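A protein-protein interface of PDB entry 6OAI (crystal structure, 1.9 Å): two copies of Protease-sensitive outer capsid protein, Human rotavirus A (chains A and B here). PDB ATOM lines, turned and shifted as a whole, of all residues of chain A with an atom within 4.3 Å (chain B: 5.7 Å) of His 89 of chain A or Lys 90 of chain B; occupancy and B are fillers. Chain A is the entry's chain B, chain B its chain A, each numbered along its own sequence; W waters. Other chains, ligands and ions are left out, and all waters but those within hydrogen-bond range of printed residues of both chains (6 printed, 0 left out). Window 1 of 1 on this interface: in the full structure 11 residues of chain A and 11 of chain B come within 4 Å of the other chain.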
ATOM      1  N   GLU A  67     -21.652 -11.467  -9.702  1.00  0.00           N
ATOM      2  CA  GLU A  67     -20.218 -11.161  -9.787  1.00  0.00           C
ATOM      3  C   GLU A  67     -20.101  -9.684 -10.169  1.00  0.00           C
ATOM      4  O   GLU A  67     -20.850  -9.230 -11.017  1.00  0.00           O
ATOM      5  CB  GLU A  67     -19.563 -12.060 -10.839  1.00  0.00           C
ATOM      6  CG  GLU A  67     -18.096 -11.780 -11.019  1.00  0.00           C
ATOM      7  CD  GLU A  67     -17.460 -12.640 -12.077  1.00  0.00           C
ATOM      8  OE1 GLU A  67     -17.646 -12.309 -13.282  1.00  0.00           O
ATOM      9  OE2 GLU A  67     -16.802 -13.609 -11.716  1.00  0.00           O
ATOM     10  N   PHE A  76     -28.471  -5.505 -10.911  1.00  0.00           N
ATOM     11  CA  PHE A  76     -28.921  -6.703 -11.683  1.00  0.00           C
ATOM     12  C   PHE A  76     -30.441  -6.577 -11.859  1.00  0.00           C
ATOM     13  O   PHE A  76     -31.153  -6.483 -10.843  1.00  0.00           O
ATOM     14  CB  PHE A  76     -28.519  -8.017 -10.990  1.00  0.00           C
ATOM     15  CG  PHE A  76     -27.089  -8.473 -11.186  1.00  0.00           C
ATOM     16  CD1 PHE A  76     -26.019  -7.617 -10.972  1.00  0.00           C
ATOM     17  CD2 PHE A  76     -26.816  -9.805 -11.476  1.00  0.00           C
ATOM     18  CE1 PHE A  76     -24.716  -8.091 -11.030  1.00  0.00           C
ATOM     19  CE2 PHE A  76     -25.517 -10.243 -11.653  1.00  0.00           C
ATOM     20  CZ  PHE A  76     -24.469  -9.397 -11.410  1.00  0.00           C
ATOM     21  N   GLU A  77     -30.898  -6.420 -13.097  1.00  0.00           N
ATOM     22  CA  GLU A  77     -32.320  -6.451 -13.419  1.00  0.00           C
ATOM     23  C   GLU A  77     -32.776  -7.897 -13.613  1.00  0.00           C
ATOM     24  O   GLU A  77     -32.452  -8.488 -14.652  1.00  0.00           O
ATOM     25  CB  GLU A  77     -32.642  -5.542 -14.573  1.00  0.00           C
ATOM     26  CG  GLU A  77     -34.108  -5.618 -14.909  1.00  0.00           C
ATOM     27  CD  GLU A  77     -34.433  -4.703 -16.066  1.00  0.00           C
ATOM     28  OE1 GLU A  77     -33.837  -3.621 -16.135  1.00  0.00           O
ATOM     29  OE2 GLU A  77     -35.315  -5.037 -16.837  1.00  0.00           O
ATOM     30  N   MET A  78     -33.559  -8.413 -12.637  1.00  0.00           N
ATOM     31  CA  MET A  78     -34.093  -9.781 -12.668  1.00  0.00           C
ATOM     32  C   MET A  78     -35.545  -9.714 -13.147  1.00  0.00           C
ATOM     33  O   MET A  78     -36.276  -8.782 -12.725  1.00  0.00           O
ATOM     34  CB  MET A  78     -33.992 -10.438 -11.289  1.00  0.00           C
ATOM     35  CG  MET A  78     -32.667 -10.360 -10.661  1.00  0.00           C
ATOM     36  SD  MET A  78     -31.359 -11.173 -11.550  1.00  0.00           S
ATOM     37  CE  MET A  78     -31.942 -12.861 -11.705  1.00  0.00           C
ATOM     38  N   GLN A  88     -34.850 -14.616 -14.642  1.00  0.00           N
ATOM     39  CA  GLN A  88     -33.617 -14.493 -15.468  1.00  0.00           C
ATOM     40  C   GLN A  88     -32.972 -13.124 -15.218  1.00  0.00           C
ATOM     41  O   GLN A  88     -33.668 -12.144 -14.817  1.00  0.00           O
ATOM     42  CB  GLN A  88     -33.935 -14.693 -16.948  1.00  0.00           C
ATOM     43  CG  GLN A  88     -34.251 -16.147 -17.333  1.00  0.00           C
ATOM     44  CD  GLN A  88     -34.315 -16.338 -18.848  1.00  0.00           C
ATOM     45  OE1 GLN A  88     -34.149 -15.373 -19.638  1.00  0.00           O
ATOM     46  NE2 GLN A  88     -34.462 -17.600 -19.267  1.00  0.00           N
ATOM     47  N   HIS A  89     -31.661 -13.089 -15.300  1.00  0.00           N
ATOM     48  CA  HIS A  89     -30.846 -11.865 -15.248  1.00  0.00           C
ATOM     49  C   HIS A  89     -30.929 -11.216 -16.622  1.00  0.00           C
ATOM     50  O   HIS A  89     -30.188 -11.659 -17.546  1.00  0.00           O
ATOM     51  CB  HIS A  89     -29.414 -12.184 -14.849  1.00  0.00           C
ATOM     52  CG  HIS A  89     -28.551 -10.984 -14.797  1.00  0.00           C
ATOM     53  ND1 HIS A  89     -27.202 -11.060 -14.851  1.00  0.00           N
ATOM     54  CD2 HIS A  89     -28.849  -9.641 -14.744  1.00  0.00           C
ATOM     55  CE1 HIS A  89     -26.677  -9.854 -14.888  1.00  0.00           C
ATOM     56  NE2 HIS A  89     -27.661  -8.952 -14.853  1.00  0.00           N
ATOM     57  N   LYS A  90     -31.862 -10.285 -16.776  1.00  0.00           N
ATOM     58  CA  LYS A  90     -32.176  -9.702 -18.101  1.00  0.00           C
ATOM     59  C   LYS A  90     -31.156  -8.624 -18.473  1.00  0.00           C
ATOM     60  O   LYS A  90     -30.793  -8.562 -19.638  1.00  0.00           O
ATOM     61  CB  LYS A  90     -33.601  -9.176 -18.104  1.00  0.00           C
ATOM     62  CG  LYS A  90     -34.167  -8.952 -19.485  1.00  0.00           C
ATOM     63  CD  LYS A  90     -35.596  -8.525 -19.427  1.00  0.00           C
ATOM     64  CE  LYS A  90     -36.124  -8.132 -20.789  1.00  0.00           C
ATOM     65  NZ  LYS A  90     -37.593  -7.980 -20.759  1.00  0.00           N
ATOM     66  N   ARG A  91     -30.828  -7.719 -17.563  1.00  0.00           N
ATOM     67  CA  ARG A  91     -30.051  -6.493 -17.864  1.00  0.00           C
ATOM     68  C   ARG A  91     -29.184  -6.128 -16.676  1.00  0.00           C
ATOM     69  O   ARG A  91     -29.360  -6.728 -15.547  1.00  0.00           O
ATOM     70  CB  ARG A  91     -30.981  -5.318 -18.190  1.00  0.00           C
ATOM     71  CG  ARG A  91     -31.952  -5.600 -19.304  1.00  0.00           C
ATOM     72  CD  ARG A  91     -32.609  -4.364 -19.907  1.00  0.00           C
ATOM     73  NE  ARG A  91     -34.013  -4.244 -19.559  1.00  0.00           N
ATOM     74  CZ  ARG A  91     -35.062  -4.462 -20.362  1.00  0.00           C
ATOM     75  NH1 ARG A  91     -34.944  -4.700 -21.658  1.00  0.00           N
ATOM     76  NH2 ARG A  91     -36.262  -4.310 -19.860  1.00  0.00           N
ATOM     77  N   THR A  92     -28.165  -5.314 -16.913  1.00  0.00           N
ATOM     78  CA  THR A  92     -27.284  -4.796 -15.848  1.00  0.00           C
ATOM     79  C   THR A  92     -27.122  -3.290 -16.031  1.00  0.00           C
ATOM     80  O   THR A  92     -26.873  -2.862 -17.161  1.00  0.00           O
ATOM     81  CB  THR A  92     -25.909  -5.475 -15.863  1.00  0.00           C
ATOM     82  OG1 THR A  92     -26.080  -6.894 -15.834  1.00  0.00           O
ATOM     83  CG2 THR A  92     -25.070  -5.058 -14.684  1.00  0.00           C
ATOM     84  N   GLU B  77     -24.346 -13.776 -23.635  1.00  0.00           N
ATOM     85  CA  GLU B  77     -23.252 -14.512 -23.009  1.00  0.00           C
ATOM     86  C   GLU B  77     -23.816 -15.314 -21.839  1.00  0.00           C
ATOM     87  O   GLU B  77     -24.165 -14.697 -20.778  1.00  0.00           O
ATOM     88  CB  GLU B  77     -22.133 -13.597 -22.547  1.00  0.00           C
ATOM     89  CG  GLU B  77     -21.061 -14.380 -21.831  1.00  0.00           C
ATOM     90  CD  GLU B  77     -19.866 -13.526 -21.488  1.00  0.00           C
ATOM     91  OE1 GLU B  77     -19.571 -12.587 -22.275  1.00  0.00           O
ATOM     92  OE2 GLU B  77     -19.305 -13.730 -20.406  1.00  0.00           O
ATOM     93  N   MET B  78     -23.948 -16.621 -22.051  1.00  0.00           N
ATOM     94  CA  MET B  78     -24.468 -17.569 -21.042  1.00  0.00           C
ATOM     95  C   MET B  78     -23.274 -18.171 -20.300  1.00  0.00           C
ATOM     96  O   MET B  78     -22.270 -18.504 -20.952  1.00  0.00           O
ATOM     97  CB  MET B  78     -25.296 -18.690 -21.703  1.00  0.00           C
ATOM     98  CG  MET B  78     -26.452 -18.196 -22.578  1.00  0.00           C
ATOM     99  SD  MET B  78     -27.530 -17.020 -21.725  1.00  0.00           S
ATOM    100  CE  MET B  78     -28.297 -18.118 -20.518  1.00  0.00           C
ATOM    101  N   PHE B  79     -23.360 -18.288 -18.983  1.00  0.00           N
ATOM    102  CA  PHE B  79     -22.221 -18.698 -18.122  1.00  0.00           C
ATOM    103  C   PHE B  79     -22.643 -19.690 -17.041  1.00  0.00           C
ATOM    104  O   PHE B  79     -23.742 -19.525 -16.434  1.00  0.00           O
ATOM    105  CB  PHE B  79     -21.615 -17.458 -17.464  1.00  0.00           C
ATOM    106  CG  PHE B  79     -20.319 -17.715 -16.754  1.00  0.00           C
ATOM    107  CD1 PHE B  79     -19.125 -17.779 -17.474  1.00  0.00           C
ATOM    108  CD2 PHE B  79     -20.283 -17.885 -15.380  1.00  0.00           C
ATOM    109  CE1 PHE B  79     -17.935 -18.035 -16.833  1.00  0.00           C
ATOM    110  CE2 PHE B  79     -19.073 -18.118 -14.732  1.00  0.00           C
ATOM    111  CZ  PHE B  79     -17.910 -18.173 -15.455  1.00  0.00           C
ATOM    112  N   GLN B  88     -26.577 -19.019 -16.512  1.00  0.00           N
ATOM    113  CA  GLN B  88     -27.153 -17.674 -16.259  1.00  0.00           C
ATOM    114  C   GLN B  88     -26.791 -16.740 -17.426  1.00  0.00           C
ATOM    115  O   GLN B  88     -25.718 -16.905 -18.049  1.00  0.00           O
ATOM    116  CB  GLN B  88     -26.647 -17.164 -14.897  1.00  0.00           C
ATOM    117  CG  GLN B  88     -27.395 -17.763 -13.681  1.00  0.00           C
ATOM    118  CD  GLN B  88     -27.146 -17.028 -12.375  1.00  0.00           C
ATOM    119  OE1 GLN B  88     -26.546 -15.943 -12.349  1.00  0.00           O
ATOM    120  NE2 GLN B  88     -27.676 -17.569 -11.283  1.00  0.00           N
ATOM    121  N   HIS B  89     -27.659 -15.806 -17.752  1.00  0.00           N
ATOM    122  CA  HIS B  89     -27.409 -14.760 -18.776  1.00  0.00           C
ATOM    123  C   HIS B  89     -26.532 -13.678 -18.132  1.00  0.00           C
ATOM    124  O   HIS B  89     -27.076 -12.834 -17.370  1.00  0.00           O
ATOM    125  CB  HIS B  89     -28.739 -14.209 -19.319  1.00  0.00           C
ATOM    126  CG  HIS B  89     -28.567 -13.103 -20.314  1.00  0.00           C
ATOM    127  ND1 HIS B  89     -29.580 -12.217 -20.621  1.00  0.00           N
ATOM    128  CD2 HIS B  89     -27.449 -12.601 -20.902  1.00  0.00           C
ATOM    129  CE1 HIS B  89     -29.126 -11.293 -21.458  1.00  0.00           C
ATOM    130  NE2 HIS B  89     -27.815 -11.529 -21.672  1.00  0.00           N
ATOM    131  N   LYS B  90     -25.216 -13.766 -18.308  1.00  0.00           N
ATOM    132  CA  LYS B  90     -24.244 -12.965 -17.533  1.00  0.00           C
ATOM    133  C   LYS B  90     -24.086 -11.590 -18.183  1.00  0.00           C
ATOM    134  O   LYS B  90     -23.947 -10.618 -17.465  1.00  0.00           O
ATOM    135  CB  LYS B  90     -22.916 -13.729 -17.501  1.00  0.00           C
ATOM    136  CG  LYS B  90     -21.830 -13.131 -16.677  1.00  0.00           C
ATOM    137  CD  LYS B  90     -20.708 -14.080 -16.327  1.00  0.00           C
ATOM    138  CE  LYS B  90     -19.698 -13.437 -15.391  1.00  0.00           C
ATOM    139  NZ  LYS B  90     -18.745 -14.414 -14.783  1.00  0.00           N
ATOM    140  N   ARG B  91     -24.033 -11.540 -19.515  1.00  0.00           N
ATOM    141  CA  ARG B  91     -23.672 -10.323 -20.265  1.00  0.00           C
ATOM    142  C   ARG B  91     -24.415 -10.304 -21.586  1.00  0.00           C
ATOM    143  O   ARG B  91     -24.968 -11.340 -22.004  1.00  0.00           O
ATOM    144  CB  ARG B  91     -22.174 -10.244 -20.574  1.00  0.00           C
ATOM    145  CG  ARG B  91     -21.338 -10.077 -19.318  1.00  0.00           C
ATOM    146  CD  ARG B  91     -19.939  -9.577 -19.567  1.00  0.00           C
ATOM    147  NE  ARG B  91     -19.088 -10.701 -19.476  1.00  0.00           N
ATOM    148  CZ  ARG B  91     -18.323 -11.039 -18.435  1.00  0.00           C
ATOM    149  NH1 ARG B  91     -18.220 -10.294 -17.348  1.00  0.00           N
ATOM    150  NH2 ARG B  91     -17.642 -12.150 -18.525  1.00  0.00           N
ATOM    151  N   THR B  92     -24.395  -9.147 -22.204  1.00  0.00           N
ATOM    152  CA  THR B  92     -25.000  -8.907 -23.499  1.00  0.00           C
ATOM    153  C   THR B  92     -24.085  -8.008 -24.309  1.00  0.00           C
ATOM    154  O   THR B  92     -23.672  -6.919 -23.781  1.00  0.00           O
ATOM    155  CB  THR B  92     -26.394  -8.311 -23.334  1.00  0.00           C
ATOM    156  OG1 THR B  92     -27.139  -9.217 -22.518  1.00  0.00           O
ATOM    157  CG2 THR B  92     -27.075  -8.143 -24.681  1.00  0.00           C
ATOM    158  N   TYR B 123     -14.162  -9.927 -17.894  1.00  0.00           N
ATOM    159  CA  TYR B 123     -13.509 -11.242 -17.763  1.00  0.00           C
ATOM    160  C   TYR B 123     -14.322 -12.175 -16.873  1.00  0.00           C
ATOM    161  O   TYR B 123     -15.125 -11.740 -16.046  1.00  0.00           O
ATOM    162  CB  TYR B 123     -12.077 -11.084 -17.281  1.00  0.00           C
ATOM    163  CG  TYR B 123     -11.906 -10.542 -15.890  1.00  0.00           C
ATOM    164  CD1 TYR B 123     -11.988 -11.362 -14.765  1.00  0.00           C
ATOM    165  CD2 TYR B 123     -11.653  -9.209 -15.704  1.00  0.00           C
ATOM    166  CE1 TYR B 123     -11.819 -10.857 -13.491  1.00  0.00           C
ATOM    167  CE2 TYR B 123     -11.543  -8.677 -14.433  1.00  0.00           C
ATOM    168  CZ  TYR B 123     -11.552  -9.527 -13.331  1.00  0.00           C
ATOM    169  OH  TYR B 123     -11.324  -9.010 -12.113  1.00  0.00           O
ATOM    170  N   SER B 124     -14.009 -13.462 -17.004  1.00  0.00           N
ATOM    171  CA  SER B 124     -14.489 -14.574 -16.168  1.00  0.00           C
ATOM    172  C   SER B 124     -13.236 -15.334 -15.699  1.00  0.00           C
ATOM    173  O   SER B 124     -12.342 -15.582 -16.500  1.00  0.00           O
ATOM    174  CB  SER B 124     -15.456 -15.450 -16.974  1.00  0.00           C
ATOM    175  OG  SER B 124     -16.762 -14.906 -17.041  1.00  0.00           O
HETATM  176  O   HOH W   1     -32.591 -12.629 -20.076  1.00  0.00           O
HETATM  177  O   HOH W   2     -30.304 -15.895 -16.050  1.00  0.00           O
HETATM  178  O   HOH W   3     -25.302 -13.540 -14.150  1.00  0.00           O
HETATM  179  O   HOH W   4     -27.865 -10.491 -18.194  1.00  0.00           O
HETATM  180  O   HOH W   5     -16.337 -15.506 -13.218  1.00  0.00           O
HETATM  181  O   HOH W   6     -18.783 -10.203 -14.187  1.00  0.00           O
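The backbone carbonyl oxygen (O) of His 89 of chain B lies within hydrogen-bond range of a ring nitrogen (ND1) of His 89 of chain A (3.1 Å).
The side-chain amino group of Lys 90 of chain B is in salt-bridge range of the side-chain carboxylate of Glu 67 of chain A (2.8 Å).
O of Glu 77 of chain B lies within hydrogen-bond range of N of Lys 90 of chain B (2.8 Å).
NE2 of His 89 of chain B is in hydrogen-bond range of OG1 of Thr 92 of chain B (2.6 Å).
The side-chain amino group (NZ) of Lys 90 of chain B lies within hydrogen-bond range of the side-chain hydroxyl (OG) of Ser 124 of chain B, at 3.0 Å.
The backbone NH (N) of Lys 90 of chain A is in hydrogen-bond range of the backbone carbonyl oxygen (O) of Glu 77 of chain A (2.8 Å).
O of Arg 91 of chain A is in hydrogen-bond range of NE2 of His 89 of chain A, at 2.9 Å.
A ring nitrogen (NE2) of His 89 of chain A is in hydrogen-bond range of the side-chain hydroxyl of Thr 92 of chain A (2.8 Å).
Among the printed residues, pairs that only touch across the chains: Lys 90 of chain A with His 89 of chain B, Glu 67 of chain A with Tyr 123 of chain B and His 89 of chain A with Lys 90 of chain B.
His 89 of chain A touches just these residues of chain B: His 89 and Lys 90.
Of chain A, only Glu 67 and His 89 come within 4 Å of Lys 90 of chain B.
Of the printed residues of chain A, Tyr 123 of chain B touches Glu 67.
Of the printed residues of chain A, His 89 of chain B touches His 89 and Lys 90.
Of the printed residues of chain B, Lys 90 of chain A touches His 89.
Arg 91 of chain A touches none of the printed residues of chain B.
Arg 91 of chain B touches none of the printed residues of chain A.
The nearest printed residue of chain A that does not touch Lys 90 of chain B is Thr 92 of chain A (4.6 Å).
The nearest printed residue of chain B that does not touch Glu 67 of chain A is Arg 91 of chain B (4.6 Å).
Of the 10 printed residues of chain B, 3 touch a printed residue of chain A.
Printed residues of chain B that touch a printed residue of chain A: His 89, Lys 90 and Tyr 123.
Among the printed residues, Asp or Glu carboxylates within 4 Å of a Lys or Arg side-chain nitrogen of the other chain: Glu 67 of chain A with Lys 90 of chain B (2.8 Å).
His 89 of chain B touches its own counterpart, His 89 of chain A.
His 89 of chain A touches Lys 90 of chain B, and with the chains exchanged Lys 90 of chain A touches His 89 of chain B.
Positions printed for both chains: 77, 78, 88, 89, 90, 91 and 92.
Water W5 lies within hydrogen-bond range of the side-chain carboxylate of Glu 67 of chain A (2.5 Å) and the side-chain amino group of Lys 90 of chain B (3.1 Å).
Water W6 lies within hydrogen-bond range of OE1 of Glu 67 of chain A and NH1 of Arg 91 of chain B.
Water W4 lies within hydrogen-bond range of O of His 89 of chain B (2.6 Å) and O of His 89 of chain A (2.7 Å).
Water W1 bridges a ring nitrogen (ND1) of His 89 of chain B (3.1 Å) and the side-chain amide oxygen of Gln 88 of chain A (3.2 Å).
Water W2 lies within hydrogen-bond range of the backbone NH (N) of His 89 of chain B (3.1 Å) and the backbone NH (N) of His 89 of chain A (3.2 Å).
Water W3 lies within hydrogen-bond range of ND1 of His 89 of chain A (3.2 Å) and OE1 of Gln 88 of chain B (3.3 Å).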
